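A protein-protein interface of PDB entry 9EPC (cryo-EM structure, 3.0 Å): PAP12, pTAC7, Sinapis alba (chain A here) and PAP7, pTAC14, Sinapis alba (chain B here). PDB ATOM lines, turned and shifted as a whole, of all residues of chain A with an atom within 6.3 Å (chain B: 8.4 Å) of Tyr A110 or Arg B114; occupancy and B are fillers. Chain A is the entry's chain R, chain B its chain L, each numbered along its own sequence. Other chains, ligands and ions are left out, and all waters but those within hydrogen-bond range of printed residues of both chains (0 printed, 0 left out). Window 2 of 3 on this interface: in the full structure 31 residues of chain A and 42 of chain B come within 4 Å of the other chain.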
ATOM      1  N   ALA A 105     -21.052   1.398  28.866  1.00  0.00           N
ATOM      2  CA  ALA A 105     -20.741   2.636  29.572  1.00  0.00           C
ATOM      3  C   ALA A 105     -20.187   3.690  28.622  1.00  0.00           C
ATOM      4  O   ALA A 105     -20.574   4.862  28.690  1.00  0.00           O
ATOM      5  CB  ALA A 105     -19.753   2.364  30.703  1.00  0.00           C
ATOM      6  N   GLU A 106     -19.281   3.292  27.728  1.00  0.00           N
ATOM      7  CA  GLU A 106     -18.712   4.247  26.784  1.00  0.00           C
ATOM      8  C   GLU A 106     -19.741   4.676  25.745  1.00  0.00           C
ATOM      9  O   GLU A 106     -19.742   5.831  25.305  1.00  0.00           O
ATOM     10  CB  GLU A 106     -17.479   3.648  26.112  1.00  0.00           C
ATOM     11  CG  GLU A 106     -16.775   4.591  25.154  1.00  0.00           C
ATOM     12  CD  GLU A 106     -15.501   3.999  24.589  1.00  0.00           C
ATOM     13  OE1 GLU A 106     -15.048   2.957  25.107  1.00  0.00           O
ATOM     14  OE2 GLU A 106     -14.951   4.576  23.628  1.00  0.00           O
ATOM     15  N   ALA A 107     -20.620   3.758  25.338  1.00  0.00           N
ATOM     16  CA  ALA A 107     -21.672   4.115  24.392  1.00  0.00           C
ATOM     17  C   ALA A 107     -22.637   5.124  24.998  1.00  0.00           C
ATOM     18  O   ALA A 107     -23.081   6.055  24.317  1.00  0.00           O
ATOM     19  CB  ALA A 107     -22.416   2.862  23.935  1.00  0.00           C
ATOM     20  N   THR A 108     -22.981   4.952  26.275  1.00  0.00           N
ATOM     21  CA  THR A 108     -23.828   5.929  26.948  1.00  0.00           C
ATOM     22  C   THR A 108     -23.140   7.285  27.022  1.00  0.00           C
ATOM     23  O   THR A 108     -23.787   8.329  26.891  1.00  0.00           O
ATOM     24  CB  THR A 108     -24.194   5.437  28.347  1.00  0.00           C
ATOM     25  OG1 THR A 108     -24.770   4.128  28.259  1.00  0.00           O
ATOM     26  CG2 THR A 108     -25.193   6.375  28.999  1.00  0.00           C
ATOM     27  N   GLU A 109     -21.823   7.288  27.235  1.00  0.00           N
ATOM     28  CA  GLU A 109     -21.080   8.541  27.260  1.00  0.00           C
ATOM     29  C   GLU A 109     -21.128   9.239  25.906  1.00  0.00           C
ATOM     30  O   GLU A 109     -21.243  10.469  25.840  1.00  0.00           O
ATOM     31  CB  GLU A 109     -19.636   8.280  27.682  1.00  0.00           C
ATOM     32  CG  GLU A 109     -18.776   9.526  27.767  1.00  0.00           C
ATOM     33  CD  GLU A 109     -17.365   9.224  28.231  1.00  0.00           C
ATOM     34  OE1 GLU A 109     -17.051   8.034  28.449  1.00  0.00           O
ATOM     35  OE2 GLU A 109     -16.570  10.176  28.380  1.00  0.00           O
ATOM     36  N   TYR A 110     -21.035   8.474  24.817  1.00  0.00           N
ATOM     37  CA  TYR A 110     -21.057   9.073  23.486  1.00  0.00           C
ATOM     38  C   TYR A 110     -22.388   9.761  23.208  1.00  0.00           C
ATOM     39  O   TYR A 110     -22.424  10.886  22.698  1.00  0.00           O
ATOM     40  CB  TYR A 110     -20.784   8.013  22.419  1.00  0.00           C
ATOM     41  CG  TYR A 110     -19.339   7.590  22.294  1.00  0.00           C
ATOM     42  CD1 TYR A 110     -18.378   8.052  23.180  1.00  0.00           C
ATOM     43  CD2 TYR A 110     -18.937   6.735  21.278  1.00  0.00           C
ATOM     44  CE1 TYR A 110     -17.057   7.664  23.063  1.00  0.00           C
ATOM     45  CE2 TYR A 110     -17.621   6.345  21.153  1.00  0.00           C
ATOM     46  CZ  TYR A 110     -16.685   6.812  22.047  1.00  0.00           C
ATOM     47  OH  TYR A 110     -15.372   6.424  21.925  1.00  0.00           O
ATOM     48  N   VAL A 111     -23.498   9.095  23.536  1.00  0.00           N
ATOM     49  CA  VAL A 111     -24.807   9.634  23.184  1.00  0.00           C
ATOM     50  C   VAL A 111     -25.136  10.861  24.027  1.00  0.00           C
ATOM     51  O   VAL A 111     -25.838  11.769  23.565  1.00  0.00           O
ATOM     52  CB  VAL A 111     -25.889   8.544  23.306  1.00  0.00           C
ATOM     53  CG1 VAL A 111     -26.127   8.163  24.755  1.00  0.00           C
ATOM     54  CG2 VAL A 111     -27.181   9.000  22.650  1.00  0.00           C
ATOM     55  N   GLU A 112     -24.643  10.917  25.267  1.00  0.00           N
ATOM     56  CA  GLU A 112     -24.893  12.086  26.104  1.00  0.00           C
ATOM     57  C   GLU A 112     -24.233  13.332  25.528  1.00  0.00           C
ATOM     58  O   GLU A 112     -24.830  14.416  25.536  1.00  0.00           O
ATOM     59  CB  GLU A 112     -24.404  11.827  27.527  1.00  0.00           C
ATOM     60  CG  GLU A 112     -25.264  10.847  28.306  1.00  0.00           C
ATOM     61  CD  GLU A 112     -24.679  10.505  29.661  1.00  0.00           C
ATOM     62  OE1 GLU A 112     -23.503  10.845  29.905  1.00  0.00           O
ATOM     63  OE2 GLU A 112     -25.396   9.893  30.482  1.00  0.00           O
ATOM     64  N   LYS A 113     -23.005  13.202  25.023  1.00  0.00           N
ATOM     65  CA  LYS A 113     -22.319  14.354  24.447  1.00  0.00           C
ATOM     66  C   LYS A 113     -22.999  14.820  23.166  1.00  0.00           C
ATOM     67  O   LYS A 113     -23.264  16.014  22.991  1.00  0.00           O
ATOM     68  CB  LYS A 113     -20.853  14.019  24.183  1.00  0.00           C
ATOM     69  CG  LYS A 113     -19.982  14.022  25.423  1.00  0.00           C
ATOM     70  CD  LYS A 113     -18.509  13.998  25.050  1.00  0.00           C
ATOM     71  CE  LYS A 113     -17.627  14.189  26.270  1.00  0.00           C
ATOM     72  NZ  LYS A 113     -16.184  14.225  25.908  1.00  0.00           N
ATOM     73  N   ASN A 114     -23.294  13.892  22.260  1.00  0.00           N
ATOM     74  CA  ASN A 114     -23.884  14.209  20.962  1.00  0.00           C
ATOM     75  C   ASN A 114     -25.193  13.440  20.837  1.00  0.00           C
ATOM     76  O   ASN A 114     -25.224  12.321  20.320  1.00  0.00           O
ATOM     77  CB  ASN A 114     -22.923  13.871  19.832  1.00  0.00           C
ATOM     78  CG  ASN A 114     -21.582  14.556  19.988  1.00  0.00           C
ATOM     79  OD1 ASN A 114     -20.704  14.070  20.701  1.00  0.00           O
ATOM     80  ND2 ASN A 114     -21.417  15.691  19.322  1.00  0.00           N
ATOM     81  N   ARG A 115     -26.278  14.049  21.319  1.00  0.00           N
ATOM     82  CA  ARG A 115     -27.585  13.409  21.237  1.00  0.00           C
ATOM     83  C   ARG A 115     -28.013  13.204  19.790  1.00  0.00           C
ATOM     84  O   ARG A 115     -28.517  12.133  19.431  1.00  0.00           O
ATOM     85  CB  ARG A 115     -28.622  14.246  21.985  1.00  0.00           C
ATOM     86  CG  ARG A 115     -28.414  14.303  23.486  1.00  0.00           C
ATOM     87  CD  ARG A 115     -28.970  13.064  24.160  1.00  0.00           C
ATOM     88  NE  ARG A 115     -30.396  12.907  23.899  1.00  0.00           N
ATOM     89  CZ  ARG A 115     -31.354  13.506  24.593  1.00  0.00           C
ATOM     90  NH1 ARG A 115     -31.074  14.312  25.604  1.00  0.00           N
ATOM     91  NH2 ARG A 115     -32.624  13.292  24.264  1.00  0.00           N
ATOM     92  N   GLU A 117     -26.659  12.513  16.973  1.00  0.00           N
ATOM     93  CA  GLU A 117     -25.780  11.840  16.025  1.00  0.00           C
ATOM     94  C   GLU A 117     -26.040  10.346  15.930  1.00  0.00           C
ATOM     95  O   GLU A 117     -25.987   9.788  14.832  1.00  0.00           O
ATOM     96  CB  GLU A 117     -24.311  12.093  16.404  1.00  0.00           C
ATOM     97  CG  GLU A 117     -23.306  11.495  15.435  1.00  0.00           C
ATOM     98  CD  GLU A 117     -21.871  11.762  15.843  1.00  0.00           C
ATOM     99  OE1 GLU A 117     -21.653  12.598  16.746  1.00  0.00           O
ATOM    100  OE2 GLU A 117     -20.959  11.136  15.263  1.00  0.00           O
ATOM    101  N   TYR A 118     -26.325   9.686  17.047  1.00  0.00           N
ATOM    102  CA  TYR A 118     -26.478   8.233  17.076  1.00  0.00           C
ATOM    103  C   TYR A 118     -27.952   7.837  17.079  1.00  0.00           C
ATOM    104  O   TYR A 118     -28.461   7.238  18.025  1.00  0.00           O
ATOM    105  CB  TYR A 118     -25.748   7.656  18.284  1.00  0.00           C
ATOM    106  CG  TYR A 118     -24.360   8.214  18.470  1.00  0.00           C
ATOM    107  CD1 TYR A 118     -23.304   7.773  17.689  1.00  0.00           C
ATOM    108  CD2 TYR A 118     -24.106   9.183  19.427  1.00  0.00           C
ATOM    109  CE1 TYR A 118     -22.035   8.281  17.855  1.00  0.00           C
ATOM    110  CE2 TYR A 118     -22.839   9.696  19.601  1.00  0.00           C
ATOM    111  CZ  TYR A 118     -21.807   9.242  18.813  1.00  0.00           C
ATOM    112  OH  TYR A 118     -20.541   9.752  18.982  1.00  0.00           O
ATOM    113  N   ALA A 124     -24.649   4.223  18.503  1.00  0.00           N
ATOM    114  CA  ALA A 124     -23.703   4.546  19.565  1.00  0.00           C
ATOM    115  C   ALA A 124     -22.779   3.370  19.852  1.00  0.00           C
ATOM    116  O   ALA A 124     -21.561   3.539  19.987  1.00  0.00           O
ATOM    117  CB  ALA A 124     -24.454   4.962  20.827  1.00  0.00           C
ATOM    118  N   HIS A 127     -20.270   2.722  17.030  1.00  0.00           N
ATOM    119  CA  HIS A 127     -19.207   3.720  17.040  1.00  0.00           C
ATOM    120  C   HIS A 127     -18.144   3.374  18.074  1.00  0.00           C
ATOM    121  O   HIS A 127     -16.948   3.578  17.838  1.00  0.00           O
ATOM    122  CB  HIS A 127     -19.786   5.107  17.308  1.00  0.00           C
ATOM    123  CG  HIS A 127     -18.828   6.220  17.021  1.00  0.00           C
ATOM    124  ND1 HIS A 127     -18.975   7.483  17.551  1.00  0.00           N
ATOM    125  CD2 HIS A 127     -17.713   6.261  16.257  1.00  0.00           C
ATOM    126  CE1 HIS A 127     -17.989   8.253  17.128  1.00  0.00           C
ATOM    127  NE2 HIS A 127     -17.209   7.536  16.341  1.00  0.00           N
ATOM    128  N   VAL A 128     -18.564   2.857  19.229  1.00  0.00           N
ATOM    129  CA  VAL A 128     -17.606   2.430  20.247  1.00  0.00           C
ATOM    130  C   VAL A 128     -16.743   1.295  19.717  1.00  0.00           C
ATOM    131  O   VAL A 128     -15.515   1.305  19.859  1.00  0.00           O
ATOM    132  CB  VAL A 128     -18.340   2.022  21.533  1.00  0.00           C
ATOM    133  CG1 VAL A 128     -17.352   1.512  22.563  1.00  0.00           C
ATOM    134  CG2 VAL A 128     -19.118   3.191  22.081  1.00  0.00           C
ATOM    135  N   ASN A 131     -14.288   2.533  17.153  1.00  0.00           N
ATOM    136  CA  ASN A 131     -13.210   3.278  17.795  1.00  0.00           C
ATOM    137  C   ASN A 131     -12.231   2.349  18.499  1.00  0.00           C
ATOM    138  O   ASN A 131     -11.014   2.535  18.400  1.00  0.00           O
ATOM    139  CB  ASN A 131     -13.786   4.289  18.784  1.00  0.00           C
ATOM    140  CG  ASN A 131     -14.503   5.428  18.095  1.00  0.00           C
ATOM    141  OD1 ASN A 131     -14.803   5.356  16.905  1.00  0.00           O
ATOM    142  ND2 ASN A 131     -14.781   6.489  18.840  1.00  0.00           N
ATOM    143  N   ARG A 132     -12.740   1.342  19.210  1.00  0.00           N
ATOM    144  CA  ARG A 132     -11.858   0.444  19.947  1.00  0.00           C
ATOM    145  C   ARG A 132     -10.960  -0.351  19.011  1.00  0.00           C
ATOM    146  O   ARG A 132      -9.815  -0.655  19.360  1.00  0.00           O
ATOM    147  CB  ARG A 132     -12.679  -0.491  20.831  1.00  0.00           C
ATOM    148  CG  ARG A 132     -13.404   0.226  21.955  1.00  0.00           C
ATOM    149  CD  ARG A 132     -14.314  -0.714  22.716  1.00  0.00           C
ATOM    150  NE  ARG A 132     -13.827  -0.979  24.063  1.00  0.00           N
ATOM    151  CZ  ARG A 132     -14.234  -0.332  25.145  1.00  0.00           C
ATOM    152  NH1 ARG A 132     -15.132   0.635  25.075  1.00  0.00           N
ATOM    153  NH2 ARG A 132     -13.729  -0.665  26.329  1.00  0.00           N
ATOM    154  N   ASP A 135      -8.382   2.122  17.854  1.00  0.00           N
ATOM    155  CA  ASP A 135      -7.396   2.357  18.901  1.00  0.00           C
ATOM    156  C   ASP A 135      -6.270   1.336  18.849  1.00  0.00           C
ATOM    157  O   ASP A 135      -5.122   1.665  19.166  1.00  0.00           O
ATOM    158  CB  ASP A 135      -8.066   2.333  20.272  1.00  0.00           C
ATOM    159  CG  ASP A 135      -9.016   3.490  20.474  1.00  0.00           C
ATOM    160  OD1 ASP A 135      -9.076   4.372  19.592  1.00  0.00           O
ATOM    161  OD2 ASP A 135      -9.705   3.517  21.513  1.00  0.00           O
ATOM    162  N   GLU B 111       0.153   7.403  14.139  1.00  0.00           N
ATOM    163  CA  GLU B 111      -0.656   8.437  14.767  1.00  0.00           C
ATOM    164  C   GLU B 111      -1.184   7.931  16.105  1.00  0.00           C
ATOM    165  O   GLU B 111      -1.794   6.856  16.157  1.00  0.00           O
ATOM    166  CB  GLU B 111      -1.807   8.840  13.848  1.00  0.00           C
ATOM    167  CG  GLU B 111      -2.436  10.185  14.179  1.00  0.00           C
ATOM    168  CD  GLU B 111      -3.505  10.086  15.248  1.00  0.00           C
ATOM    169  OE1 GLU B 111      -4.208   9.056  15.295  1.00  0.00           O
ATOM    170  OE2 GLU B 111      -3.641  11.040  16.043  1.00  0.00           O
ATOM    171  N   PRO B 112      -0.969   8.658  17.198  1.00  0.00           N
ATOM    172  CA  PRO B 112      -1.380   8.154  18.512  1.00  0.00           C
ATOM    173  C   PRO B 112      -2.890   8.049  18.633  1.00  0.00           C
ATOM    174  O   PRO B 112      -3.645   8.838  18.060  1.00  0.00           O
ATOM    175  CB  PRO B 112      -0.819   9.200  19.481  1.00  0.00           C
ATOM    176  CG  PRO B 112      -0.757  10.448  18.676  1.00  0.00           C
ATOM    177  CD  PRO B 112      -0.414  10.018  17.276  1.00  0.00           C
ATOM    178  N   ARG B 113      -3.327   7.058  19.399  1.00  0.00           N
ATOM    179  CA  ARG B 113      -4.739   6.800  19.635  1.00  0.00           C
ATOM    180  C   ARG B 113      -5.021   6.893  21.133  1.00  0.00           C
ATOM    181  O   ARG B 113      -4.155   7.265  21.928  1.00  0.00           O
ATOM    182  CB  ARG B 113      -5.135   5.436  19.065  1.00  0.00           C
ATOM    183  CG  ARG B 113      -4.680   5.212  17.636  1.00  0.00           C
ATOM    184  CD  ARG B 113      -5.308   6.216  16.689  1.00  0.00           C
ATOM    185  NE  ARG B 113      -4.729   6.135  15.355  1.00  0.00           N
ATOM    186  CZ  ARG B 113      -5.126   5.288  14.415  1.00  0.00           C
ATOM    187  NH1 ARG B 113      -6.105   4.426  14.631  1.00  0.00           N
ATOM    188  NH2 ARG B 113      -4.522   5.304  13.231  1.00  0.00           N
ATOM    189  N   ARG B 114      -6.254   6.553  21.516  1.00  0.00           N
ATOM    190  CA  ARG B 114      -6.616   6.581  22.929  1.00  0.00           C
ATOM    191  C   ARG B 114      -5.811   5.563  23.724  1.00  0.00           C
ATOM    192  O   ARG B 114      -5.365   5.846  24.841  1.00  0.00           O
ATOM    193  CB  ARG B 114      -8.114   6.322  23.100  1.00  0.00           C
ATOM    194  CG  ARG B 114      -8.604   6.531  24.524  1.00  0.00           C
ATOM    195  CD  ARG B 114      -9.992   5.954  24.755  1.00  0.00           C
ATOM    196  NE  ARG B 114     -10.966   6.424  23.776  1.00  0.00           N
ATOM    197  CZ  ARG B 114     -11.574   5.645  22.892  1.00  0.00           C
ATOM    198  NH1 ARG B 114     -11.349   4.343  22.847  1.00  0.00           N
ATOM    199  NH2 ARG B 114     -12.435   6.187  22.035  1.00  0.00           N
ATOM    200  N   ARG B 115      -5.610   4.375  23.166  1.00  0.00           N
ATOM    201  CA  ARG B 115      -4.933   3.283  23.847  1.00  0.00           C
ATOM    202  C   ARG B 115      -3.725   2.840  23.024  1.00  0.00           C
ATOM    203  O   ARG B 115      -3.485   3.326  21.917  1.00  0.00           O
ATOM    204  CB  ARG B 115      -5.907   2.124  24.097  1.00  0.00           C
ATOM    205  CG  ARG B 115      -5.465   1.146  25.178  1.00  0.00           C
ATOM    206  CD  ARG B 115      -4.869   1.881  26.369  1.00  0.00           C
ATOM    207  NE  ARG B 115      -4.009   1.020  27.171  1.00  0.00           N
ATOM    208  CZ  ARG B 115      -3.276   1.438  28.194  1.00  0.00           C
ATOM    209  NH1 ARG B 115      -3.279   2.705  28.574  1.00  0.00           N
ATOM    210  NH2 ARG B 115      -2.521   0.563  28.852  1.00  0.00           N
ATOM    211  N   ALA B 116      -2.955   1.913  23.591  1.00  0.00           N
ATOM    212  CA  ALA B 116      -1.755   1.413  22.936  1.00  0.00           C
ATOM    213  C   ALA B 116      -2.099   0.739  21.615  1.00  0.00           C
ATOM    214  O   ALA B 116      -3.137   0.086  21.482  1.00  0.00           O
ATOM    215  CB  ALA B 116      -1.031   0.429  23.854  1.00  0.00           C
ATOM    216  N   ARG B 117      -1.218   0.902  20.634  1.00  0.00           N
ATOM    217  CA  ARG B 117      -1.410   0.336  19.308  1.00  0.00           C
ATOM    218  C   ARG B 117      -0.585  -0.933  19.157  1.00  0.00           C
ATOM    219  O   ARG B 117       0.580  -0.983  19.561  1.00  0.00           O
ATOM    220  CB  ARG B 117      -1.020   1.339  18.223  1.00  0.00           C
ATOM    221  CG  ARG B 117      -1.834   2.616  18.244  1.00  0.00           C
ATOM    222  CD  ARG B 117      -1.495   3.499  17.058  1.00  0.00           C
ATOM    223  NE  ARG B 117      -1.682   2.798  15.794  1.00  0.00           N
ATOM    224  CZ  ARG B 117      -1.589   3.365  14.601  1.00  0.00           C
ATOM    225  NH1 ARG B 117      -1.310   4.651  14.467  1.00  0.00           N
ATOM    226  NH2 ARG B 117      -1.784   2.625  13.513  1.00  0.00           N
ATOM    227  N   ASN B 309       3.537   2.680  23.205  1.00  0.00           N
ATOM    228  CA  ASN B 309       2.960   3.374  24.348  1.00  0.00           C
ATOM    229  C   ASN B 309       1.742   4.187  23.925  1.00  0.00           C
ATOM    230  O   ASN B 309       1.735   4.825  22.870  1.00  0.00           O
ATOM    231  CB  ASN B 309       4.001   4.283  24.997  1.00  0.00           C
ATOM    232  CG  ASN B 309       5.188   3.514  25.531  1.00  0.00           C
ATOM    233  OD1 ASN B 309       6.320   3.723  25.102  1.00  0.00           O
ATOM    234  ND2 ASN B 309       4.936   2.615  26.474  1.00  0.00           N
ATOM    235  N   ALA B 310       0.705   4.150  24.757  1.00  0.00           N
ATOM    236  CA  ALA B 310      -0.548   4.812  24.424  1.00  0.00           C
ATOM    237  C   ALA B 310      -0.362   6.321  24.357  1.00  0.00           C
ATOM    238  O   ALA B 310       0.334   6.917  25.183  1.00  0.00           O
ATOM    239  CB  ALA B 310      -1.621   4.461  25.453  1.00  0.00           C
ATOM    240  N   GLY B 311      -0.990   6.937  23.359  1.00  0.00           N
ATOM    241  CA  GLY B 311      -0.926   8.376  23.215  1.00  0.00           C
ATOM    242  C   GLY B 311       0.419   8.916  22.794  1.00  0.00           C
ATOM    243  O   GLY B 311       0.672  10.111  22.957  1.00  0.00           O
ATOM    244  N   GLN B 312       1.291   8.072  22.252  1.00  0.00           N
ATOM    245  CA  GLN B 312       2.609   8.488  21.797  1.00  0.00           C
ATOM    246  C   GLN B 312       2.701   8.319  20.289  1.00  0.00           C
ATOM    247  O   GLN B 312       2.362   7.258  19.757  1.00  0.00           O
ATOM    248  CB  GLN B 312       3.711   7.682  22.486  1.00  0.00           C
ATOM    249  CG  GLN B 312       5.107   8.024  21.999  1.00  0.00           C
ATOM    250  CD  GLN B 312       6.187   7.301  22.771  1.00  0.00           C
ATOM    251  OE1 GLN B 312       5.911   6.617  23.756  1.00  0.00           O
ATOM    252  NE2 GLN B 312       7.430   7.450  22.329  1.00  0.00           N
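Tyr A110 touches just one residue of chain B: Arg B114 (2.9 Å). Of the printed residues of chain B, Asn A131 touches Arg B114 (3.98 Å). Of the printed residues of chain B, Asp A135 touches Arg B113 (3.8 Å), Arg B114 (2.3 Å), Arg B115 (3.6 Å), Ala B116 (3.4 Å) and Arg B117 (3.5 Å). Of the printed residues of chain A, Arg B115 touches Asp A135. Printed residues of chain A within 4 Å of Arg B117: Asp A135.
OE1 of Glu B111 lies within salt-bridge range of NE of Arg B113 (3.0 Å). O of Glu B111 sits at hydrogen-bond distance from NH1 of Arg B117 (2.8 Å). The backbone carbonyl oxygen (O) of Arg B113 sits at hydrogen-bond distance from the backbone NH (N) of Gly B311, 3.5 Å away. OE2 of Glu A106 is in hydrogen-bond range of OH of Tyr A110, 2.5 Å away. ND2 of Asn A131 lies within hydrogen-bond range of OH of Tyr A110. The backbone carbonyl oxygen (O) of His A127 sits close to the side-chain amide oxygen (OD1) of Asn A131, 2.9 Å away.
The guanidinium group (NH2) of Arg B114 is in salt-bridge range of the side-chain carboxylate (OE2) of Glu A106, 3.4 Å away. The guanidinium group (NH2) of Arg B114 sits at hydrogen-bond distance from the side-chain hydroxyl (OH) of Tyr A110. The guanidinium group of Arg B114 lies within salt-bridge range of the side-chain carboxylate of Asp A135, at 3.9 Å. O of Ala B116 sits close to O of Asp A135 (3.4 Å).
Among the printed residues, merely in contact across the chains: Asp A135 with Arg B117 (3.5 Å), Asp A135 with Arg B115 (3.6 Å), Asp A135 with Arg B113 (3.8 Å) and Asn A131 with Arg B114 (3.98 Å).
Hydrophobic or aromatic side chains of chain A that line the printed part of chain B: Tyr A110. Of the 11 printed residues of chain B, 5 touch a printed residue of chain A. Along chain B the printed residues that touch a printed residue of chain A span positions 113 to 117.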
